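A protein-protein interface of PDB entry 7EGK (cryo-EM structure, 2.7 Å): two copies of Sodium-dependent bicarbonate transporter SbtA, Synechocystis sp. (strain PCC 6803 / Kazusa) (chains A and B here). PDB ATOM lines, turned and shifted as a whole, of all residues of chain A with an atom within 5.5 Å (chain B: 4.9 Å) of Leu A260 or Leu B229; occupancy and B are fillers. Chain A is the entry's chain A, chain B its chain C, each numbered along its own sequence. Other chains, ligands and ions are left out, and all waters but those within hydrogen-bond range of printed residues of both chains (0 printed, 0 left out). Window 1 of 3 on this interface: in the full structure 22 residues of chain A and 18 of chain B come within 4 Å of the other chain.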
ATOM      1  N   PHE A  22      23.726  -6.655  11.970  1.00  0.00           N
ATOM      2  CA  PHE A  22      24.654  -6.747  13.086  1.00  0.00           C
ATOM      3  C   PHE A  22      26.091  -6.587  12.624  1.00  0.00           C
ATOM      4  O   PHE A  22      26.950  -6.192  13.413  1.00  0.00           O
ATOM      5  CB  PHE A  22      24.465  -8.072  13.810  1.00  0.00           C
ATOM      6  CG  PHE A  22      23.303  -8.086  14.751  1.00  0.00           C
ATOM      7  CD1 PHE A  22      22.033  -8.369  14.294  1.00  0.00           C
ATOM      8  CD2 PHE A  22      23.483  -7.829  16.096  1.00  0.00           C
ATOM      9  CE1 PHE A  22      20.960  -8.389  15.159  1.00  0.00           C
ATOM     10  CE2 PHE A  22      22.415  -7.849  16.966  1.00  0.00           C
ATOM     11  CZ  PHE A  22      21.152  -8.131  16.495  1.00  0.00           C
ATOM     12  N   LEU A  23      26.372  -6.892  11.357  1.00  0.00           N
ATOM     13  CA  LEU A  23      27.676  -6.583  10.782  1.00  0.00           C
ATOM     14  C   LEU A  23      27.863  -5.080  10.636  1.00  0.00           C
ATOM     15  O   LEU A  23      28.911  -4.537  11.000  1.00  0.00           O
ATOM     16  CB  LEU A  23      27.821  -7.281   9.432  1.00  0.00           C
ATOM     17  CG  LEU A  23      28.907  -6.780   8.482  1.00  0.00           C
ATOM     18  CD1 LEU A  23      30.239  -7.368   8.830  1.00  0.00           C
ATOM     19  CD2 LEU A  23      28.549  -7.093   7.044  1.00  0.00           C
ATOM     20  N   GLY A  25      26.011  -2.842  12.244  1.00  0.00           N
ATOM     21  CA  GLY A  25      25.836  -2.240  13.556  1.00  0.00           C
ATOM     22  C   GLY A  25      27.081  -2.328  14.414  1.00  0.00           C
ATOM     23  O   GLY A  25      27.375  -1.424  15.194  1.00  0.00           O
ATOM     24  N   GLY A  26      27.837  -3.415  14.273  1.00  0.00           N
ATOM     25  CA  GLY A  26      29.122  -3.498  14.937  1.00  0.00           C
ATOM     26  C   GLY A  26      30.167  -2.599  14.328  1.00  0.00           C
ATOM     27  O   GLY A  26      31.085  -2.168  15.028  1.00  0.00           O
ATOM     28  N   MET A  27      30.040  -2.296  13.042  1.00  0.00           N
ATOM     29  CA  MET A  27      31.003  -1.442  12.368  1.00  0.00           C
ATOM     30  C   MET A  27      30.746   0.025  12.677  1.00  0.00           C
ATOM     31  O   MET A  27      31.676   0.834  12.675  1.00  0.00           O
ATOM     32  CB  MET A  27      30.935  -1.705  10.869  1.00  0.00           C
ATOM     33  CG  MET A  27      32.091  -1.207  10.061  1.00  0.00           C
ATOM     34  SD  MET A  27      31.759  -1.538   8.326  1.00  0.00           S
ATOM     35  CE  MET A  27      31.729  -3.320   8.327  1.00  0.00           C
ATOM     36  N   ILE A  29      29.270   1.225  15.646  1.00  0.00           N
ATOM     37  CA  ILE A  29      29.578   1.541  17.039  1.00  0.00           C
ATOM     38  C   ILE A  29      31.075   1.483  17.294  1.00  0.00           C
ATOM     39  O   ILE A  29      31.577   2.144  18.208  1.00  0.00           O
ATOM     40  CB  ILE A  29      28.806   0.622  18.008  1.00  0.00           C
ATOM     41  CG1 ILE A  29      29.242  -0.833  17.868  1.00  0.00           C
ATOM     42  CG2 ILE A  29      27.317   0.757  17.799  1.00  0.00           C
ATOM     43  CD1 ILE A  29      28.660  -1.744  18.907  1.00  0.00           C
ATOM     44  N   LEU A  36      32.207  -0.964  24.479  1.00  0.00           N
ATOM     45  CA  LEU A  36      31.593  -2.280  24.504  1.00  0.00           C
ATOM     46  C   LEU A  36      32.517  -3.281  23.838  1.00  0.00           C
ATOM     47  O   LEU A  36      32.912  -3.106  22.685  1.00  0.00           O
ATOM     48  CB  LEU A  36      30.240  -2.258  23.792  1.00  0.00           C
ATOM     49  CG  LEU A  36      29.666  -3.607  23.343  1.00  0.00           C
ATOM     50  CD1 LEU A  36      29.243  -4.449  24.526  1.00  0.00           C
ATOM     51  CD2 LEU A  36      28.504  -3.403  22.406  1.00  0.00           C
ATOM     52  N   ILE A  38      33.001  -7.666  23.403  1.00  0.00           N
ATOM     53  CA  ILE A  38      32.501  -9.013  23.639  1.00  0.00           C
ATOM     54  C   ILE A  38      33.695  -9.792  24.165  1.00  0.00           C
ATOM     55  O   ILE A  38      34.776  -9.708  23.572  1.00  0.00           O
ATOM     56  CB  ILE A  38      31.919  -9.639  22.363  1.00  0.00           C
ATOM     57  CG1 ILE A  38      30.821  -8.749  21.786  1.00  0.00           C
ATOM     58  CG2 ILE A  38      31.383 -11.027  22.646  1.00  0.00           C
ATOM     59  CD1 ILE A  38      29.624  -8.602  22.687  1.00  0.00           C
ATOM     60  N   LEU A 255      24.740 -16.374  15.935  1.00  0.00           N
ATOM     61  CA  LEU A 255      25.378 -15.836  14.743  1.00  0.00           C
ATOM     62  C   LEU A 255      25.270 -14.319  14.698  1.00  0.00           C
ATOM     63  O   LEU A 255      26.170 -13.643  14.189  1.00  0.00           O
ATOM     64  CB  LEU A 255      24.757 -16.470  13.503  1.00  0.00           C
ATOM     65  CG  LEU A 255      25.213 -15.998  12.130  1.00  0.00           C
ATOM     66  CD1 LEU A 255      26.636 -16.418  11.873  1.00  0.00           C
ATOM     67  CD2 LEU A 255      24.302 -16.575  11.105  1.00  0.00           C
ATOM     68  N   SER A 256      24.192 -13.763  15.250  1.00  0.00           N
ATOM     69  CA  SER A 256      24.036 -12.314  15.272  1.00  0.00           C
ATOM     70  C   SER A 256      25.025 -11.651  16.219  1.00  0.00           C
ATOM     71  O   SER A 256      25.387 -10.490  16.017  1.00  0.00           O
ATOM     72  CB  SER A 256      22.606 -11.947  15.656  1.00  0.00           C
ATOM     73  OG  SER A 256      22.357 -12.234  17.016  1.00  0.00           O
ATOM     74  N   ILE A 257      25.474 -12.358  17.253  1.00  0.00           N
ATOM     75  CA  ILE A 257      26.533 -11.825  18.098  1.00  0.00           C
ATOM     76  C   ILE A 257      27.876 -11.928  17.389  1.00  0.00           C
ATOM     77  O   ILE A 257      28.704 -11.016  17.474  1.00  0.00           O
ATOM     78  CB  ILE A 257      26.542 -12.539  19.462  1.00  0.00           C
ATOM     79  CG1 ILE A 257      25.193 -12.376  20.153  1.00  0.00           C
ATOM     80  CG2 ILE A 257      27.633 -11.998  20.363  1.00  0.00           C
ATOM     81  CD1 ILE A 257      25.113 -13.037  21.497  1.00  0.00           C
ATOM     82  N   LEU A 258      28.106 -13.022  16.659  1.00  0.00           N
ATOM     83  CA  LEU A 258      29.342 -13.161  15.895  1.00  0.00           C
ATOM     84  C   LEU A 258      29.389 -12.177  14.735  1.00  0.00           C
ATOM     85  O   LEU A 258      30.465 -11.699  14.366  1.00  0.00           O
ATOM     86  CB  LEU A 258      29.494 -14.590  15.387  1.00  0.00           C
ATOM     87  CG  LEU A 258      30.857 -14.924  14.780  1.00  0.00           C
ATOM     88  CD1 LEU A 258      31.948 -14.853  15.827  1.00  0.00           C
ATOM     89  CD2 LEU A 258      30.840 -16.269  14.112  1.00  0.00           C
ATOM     90  N   MET A 259      28.230 -11.852  14.158  1.00  0.00           N
ATOM     91  CA  MET A 259      28.170 -10.788  13.163  1.00  0.00           C
ATOM     92  C   MET A 259      28.494  -9.437  13.775  1.00  0.00           C
ATOM     93  O   MET A 259      28.997  -8.553  13.084  1.00  0.00           O
ATOM     94  CB  MET A 259      26.790 -10.734  12.517  1.00  0.00           C
ATOM     95  CG  MET A 259      26.538 -11.763  11.449  1.00  0.00           C
ATOM     96  SD  MET A 259      27.701 -11.658  10.096  1.00  0.00           S
ATOM     97  CE  MET A 259      28.405 -13.283  10.179  1.00  0.00           C
ATOM     98  N   LEU A 260      28.205  -9.250  15.059  1.00  0.00           N
ATOM     99  CA  LEU A 260      28.594  -8.013  15.721  1.00  0.00           C
ATOM    100  C   LEU A 260      30.098  -7.966  15.946  1.00  0.00           C
ATOM    101  O   LEU A 260      30.717  -6.910  15.807  1.00  0.00           O
ATOM    102  CB  LEU A 260      27.847  -7.870  17.041  1.00  0.00           C
ATOM    103  CG  LEU A 260      27.923  -6.487  17.666  1.00  0.00           C
ATOM    104  CD1 LEU A 260      26.890  -5.603  17.031  1.00  0.00           C
ATOM    105  CD2 LEU A 260      27.724  -6.577  19.155  1.00  0.00           C
ATOM    106  N   ILE A 261      30.698  -9.109  16.287  1.00  0.00           N
ATOM    107  CA  ILE A 261      32.138  -9.181  16.535  1.00  0.00           C
ATOM    108  C   ILE A 261      32.911  -8.947  15.244  1.00  0.00           C
ATOM    109  O   ILE A 261      33.810  -8.102  15.178  1.00  0.00           O
ATOM    110  CB  ILE A 261      32.506 -10.534  17.162  1.00  0.00           C
ATOM    111  CG1 ILE A 261      31.881 -10.673  18.546  1.00  0.00           C
ATOM    112  CG2 ILE A 261      34.007 -10.701  17.237  1.00  0.00           C
ATOM    113  CD1 ILE A 261      31.805 -12.094  19.026  1.00  0.00           C
ATOM    114  N   MET A 262      32.574  -9.694  14.202  1.00  0.00           N
ATOM    115  CA  MET A 262      33.146  -9.467  12.880  1.00  0.00           C
ATOM    116  C   MET A 262      32.503  -8.222  12.297  1.00  0.00           C
ATOM    117  O   MET A 262      31.426  -8.283  11.715  1.00  0.00           O
ATOM    118  CB  MET A 262      32.913 -10.672  11.979  1.00  0.00           C
ATOM    119  CG  MET A 262      33.281 -12.000  12.603  1.00  0.00           C
ATOM    120  SD  MET A 262      34.963 -12.061  13.241  1.00  0.00           S
ATOM    121  CE  MET A 262      35.904 -11.785  11.747  1.00  0.00           C
ATOM    122  N   GLY A 263      33.176  -7.093  12.412  1.00  0.00           N
ATOM    123  CA  GLY A 263      32.577  -5.817  12.086  1.00  0.00           C
ATOM    124  C   GLY A 263      33.041  -4.787  13.084  1.00  0.00           C
ATOM    125  O   GLY A 263      33.353  -3.657  12.716  1.00  0.00           O
ATOM    126  N   MET A 264      33.164  -5.184  14.344  1.00  0.00           N
ATOM    127  CA  MET A 264      34.076  -4.473  15.224  1.00  0.00           C
ATOM    128  C   MET A 264      35.508  -4.866  14.914  1.00  0.00           C
ATOM    129  O   MET A 264      36.431  -4.076  15.135  1.00  0.00           O
ATOM    130  CB  MET A 264      33.748  -4.765  16.683  1.00  0.00           C
ATOM    131  CG  MET A 264      32.344  -4.404  17.074  1.00  0.00           C
ATOM    132  SD  MET A 264      32.047  -4.602  18.825  1.00  0.00           S
ATOM    133  CE  MET A 264      32.981  -3.207  19.408  1.00  0.00           C
ATOM    134  N   GLU A 265      35.694  -6.082  14.402  1.00  0.00           N
ATOM    135  CA  GLU A 265      36.984  -6.504  13.880  1.00  0.00           C
ATOM    136  C   GLU A 265      37.356  -5.720  12.633  1.00  0.00           C
ATOM    137  O   GLU A 265      38.531  -5.414  12.415  1.00  0.00           O
ATOM    138  CB  GLU A 265      36.944  -7.992  13.554  1.00  0.00           C
ATOM    139  CG  GLU A 265      37.328  -8.878  14.684  1.00  0.00           C
ATOM    140  CD  GLU A 265      38.750  -8.666  15.098  1.00  0.00           C
ATOM    141  OE1 GLU A 265      39.657  -9.183  14.414  1.00  0.00           O
ATOM    142  OE2 GLU A 265      38.967  -7.973  16.110  1.00  0.00           O
ATOM    143  N   PHE B  48      24.855  -7.295  28.008  1.00  0.00           N
ATOM    144  CA  PHE B  48      24.670  -7.089  26.575  1.00  0.00           C
ATOM    145  C   PHE B  48      23.364  -7.703  26.091  1.00  0.00           C
ATOM    146  O   PHE B  48      22.652  -7.096  25.289  1.00  0.00           O
ATOM    147  CB  PHE B  48      25.852  -7.676  25.798  1.00  0.00           C
ATOM    148  CG  PHE B  48      25.604  -7.806  24.319  1.00  0.00           C
ATOM    149  CD1 PHE B  48      25.687  -6.699  23.499  1.00  0.00           C
ATOM    150  CD2 PHE B  48      25.294  -9.035  23.749  1.00  0.00           C
ATOM    151  CE1 PHE B  48      25.454  -6.807  22.150  1.00  0.00           C
ATOM    152  CE2 PHE B  48      25.050  -9.142  22.402  1.00  0.00           C
ATOM    153  CZ  PHE B  48      25.134  -8.029  21.602  1.00  0.00           C
ATOM    154  N   THR B  52      20.227  -5.298  24.831  1.00  0.00           N
ATOM    155  CA  THR B  52      19.913  -5.354  23.408  1.00  0.00           C
ATOM    156  C   THR B  52      18.452  -5.709  23.192  1.00  0.00           C
ATOM    157  O   THR B  52      17.811  -5.174  22.285  1.00  0.00           O
ATOM    158  CB  THR B  52      20.820  -6.357  22.700  1.00  0.00           C
ATOM    159  OG1 THR B  52      22.165  -6.161  23.139  1.00  0.00           O
ATOM    160  CG2 THR B  52      20.772  -6.168  21.207  1.00  0.00           C
ATOM    161  N   SER B 225      25.752   1.496  25.055  1.00  0.00           N
ATOM    162  CA  SER B 225      25.982   1.267  23.632  1.00  0.00           C
ATOM    163  C   SER B 225      25.213   0.053  23.137  1.00  0.00           C
ATOM    164  O   SER B 225      24.875  -0.032  21.952  1.00  0.00           O
ATOM    165  CB  SER B 225      27.467   1.084  23.357  1.00  0.00           C
ATOM    166  OG  SER B 225      28.187   2.252  23.679  1.00  0.00           O
ATOM    167  N   ALA B 226      24.944  -0.905  24.023  1.00  0.00           N
ATOM    168  CA  ALA B 226      24.181  -2.082  23.634  1.00  0.00           C
ATOM    169  C   ALA B 226      22.713  -1.744  23.432  1.00  0.00           C
ATOM    170  O   ALA B 226      22.046  -2.340  22.583  1.00  0.00           O
ATOM    171  CB  ALA B 226      24.341  -3.180  24.681  1.00  0.00           C
ATOM    172  N   MET B 227      22.191  -0.788  24.201  1.00  0.00           N
ATOM    173  CA  MET B 227      20.802  -0.383  24.029  1.00  0.00           C
ATOM    174  C   MET B 227      20.631   0.461  22.774  1.00  0.00           C
ATOM    175  O   MET B 227      19.664   0.290  22.026  1.00  0.00           O
ATOM    176  CB  MET B 227      20.316   0.378  25.258  1.00  0.00           C
ATOM    177  CG  MET B 227      18.911   0.914  25.103  1.00  0.00           C
ATOM    178  SD  MET B 227      18.297   1.798  26.522  1.00  0.00           S
ATOM    179  CE  MET B 227      17.930   0.412  27.579  1.00  0.00           C
ATOM    180  N   LEU B 228      21.576   1.373  22.521  1.00  0.00           N
ATOM    181  CA  LEU B 228      21.498   2.226  21.340  1.00  0.00           C
ATOM    182  C   LEU B 228      21.687   1.424  20.063  1.00  0.00           C
ATOM    183  O   LEU B 228      21.144   1.782  19.014  1.00  0.00           O
ATOM    184  CB  LEU B 228      22.541   3.334  21.420  1.00  0.00           C
ATOM    185  CG  LEU B 228      22.325   4.433  22.452  1.00  0.00           C
ATOM    186  CD1 LEU B 228      23.381   5.495  22.284  1.00  0.00           C
ATOM    187  CD2 LEU B 228      20.944   5.026  22.316  1.00  0.00           C
ATOM    188  N   LEU B 229      22.467   0.348  20.133  1.00  0.00           N
ATOM    189  CA  LEU B 229      22.556  -0.585  19.018  1.00  0.00           C
ATOM    190  C   LEU B 229      21.218  -1.266  18.777  1.00  0.00           C
ATOM    191  O   LEU B 229      20.770  -1.388  17.635  1.00  0.00           O
ATOM    192  CB  LEU B 229      23.642  -1.617  19.298  1.00  0.00           C
ATOM    193  CG  LEU B 229      23.663  -2.871  18.432  1.00  0.00           C
ATOM    194  CD1 LEU B 229      24.341  -2.612  17.107  1.00  0.00           C
ATOM    195  CD2 LEU B 229      24.339  -3.990  19.190  1.00  0.00           C
ATOM    196  N   GLY B 230      20.560  -1.697  19.845  1.00  0.00           N
ATOM    197  CA  GLY B 230      19.244  -2.277  19.753  1.00  0.00           C
ATOM    198  C   GLY B 230      18.159  -1.337  19.303  1.00  0.00           C
ATOM    199  O   GLY B 230      17.257  -1.767  18.582  1.00  0.00           O
ATOM    200  N   LEU B 231      18.207  -0.071  19.718  1.00  0.00           N
ATOM    201  CA  LEU B 231      17.304   0.959  19.220  1.00  0.00           C
ATOM    202  C   LEU B 231      17.430   1.167  17.722  1.00  0.00           C
ATOM    203  O   LEU B 231      16.417   1.265  17.028  1.00  0.00           O
ATOM    204  CB  LEU B 231      17.568   2.288  19.923  1.00  0.00           C
ATOM    205  CG  LEU B 231      16.630   2.770  21.022  1.00  0.00           C
ATOM    206  CD1 LEU B 231      16.709   1.893  22.227  1.00  0.00           C
ATOM    207  CD2 LEU B 231      16.980   4.186  21.397  1.00  0.00           C
ATOM    208  N   ALA B 232      18.658   1.227  17.211  1.00  0.00           N
ATOM    209  CA  ALA B 232      18.870   1.470  15.792  1.00  0.00           C
ATOM    210  C   ALA B 232      18.474   0.268  14.950  1.00  0.00           C
ATOM    211  O   ALA B 232      17.961   0.431  13.841  1.00  0.00           O
ATOM    212  CB  ALA B 232      20.328   1.840  15.538  1.00  0.00           C
ATOM    213  N   LEU B 233      18.689  -0.944  15.459  1.00  0.00           N
ATOM    214  CA  LEU B 233      18.299  -2.127  14.704  1.00  0.00           C
ATOM    215  C   LEU B 233      16.796  -2.350  14.767  1.00  0.00           C
ATOM    216  O   LEU B 233      16.225  -3.014  13.900  1.00  0.00           O
ATOM    217  CB  LEU B 233      19.045  -3.354  15.216  1.00  0.00           C
ATOM    218  CG  LEU B 233      20.556  -3.349  14.995  1.00  0.00           C
ATOM    219  CD1 LEU B 233      21.166  -4.640  15.468  1.00  0.00           C
ATOM    220  CD2 LEU B 233      20.889  -3.108  13.550  1.00  0.00           C
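Of the 11 printed residues of chain B, 3 touch a printed residue of chain A.
Hydrophobic or aromatic side chains of chain B that line the printed part of chain A: Phe B48, Leu B229 and Leu B233.
Printed residues of chain A that touch a printed residue of chain B: Phe A22, Gly A25, Ile A257 and Leu A260.
Among the printed residues, 5 pairs touch across the chains.
Among the printed residues, no Asp or Glu carboxylate lies within 4 Å of a Lys or Arg side-chain nitrogen of the other chain.
Printed residues of chain B within 4 Å of Leu A260: Phe B48 (3.8 Å) and Leu B229 (3.7 Å).
Printed residues of chain B within 4 Å of Phe A22: Leu B233.
Of the printed residues of chain A, Phe B48 touches Ile A257 and Leu A260.
Of the printed residues of chain B, Gly A25 touches Leu B229 (3.8 Å).
Ala B232 touches none of the printed residues of chain A.
Leu A23 touches none of the printed residues of chain B.
The nearest printed residue of chain B that does not touch Leu A260 is Leu B233 (6.0 Å).
The nearest printed residue of chain A that does not touch Phe B48 is Leu A36 (4.3 Å).
No position is printed for both chains.
Of the 5 pairs that touch across the chains among the printed residues, none has its exchanged pair printed and touching as well.
Among the printed residues, pairs that only touch across the chains: Phe A22 with Leu B233 (3.6 Å), Leu A260 with Leu B229 (3.7 Å), Leu A260 with Phe B48 (3.8 Å), Gly A25 with Leu B229 (3.8 Å) and Ile A257 with Phe B48 (3.9 Å).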
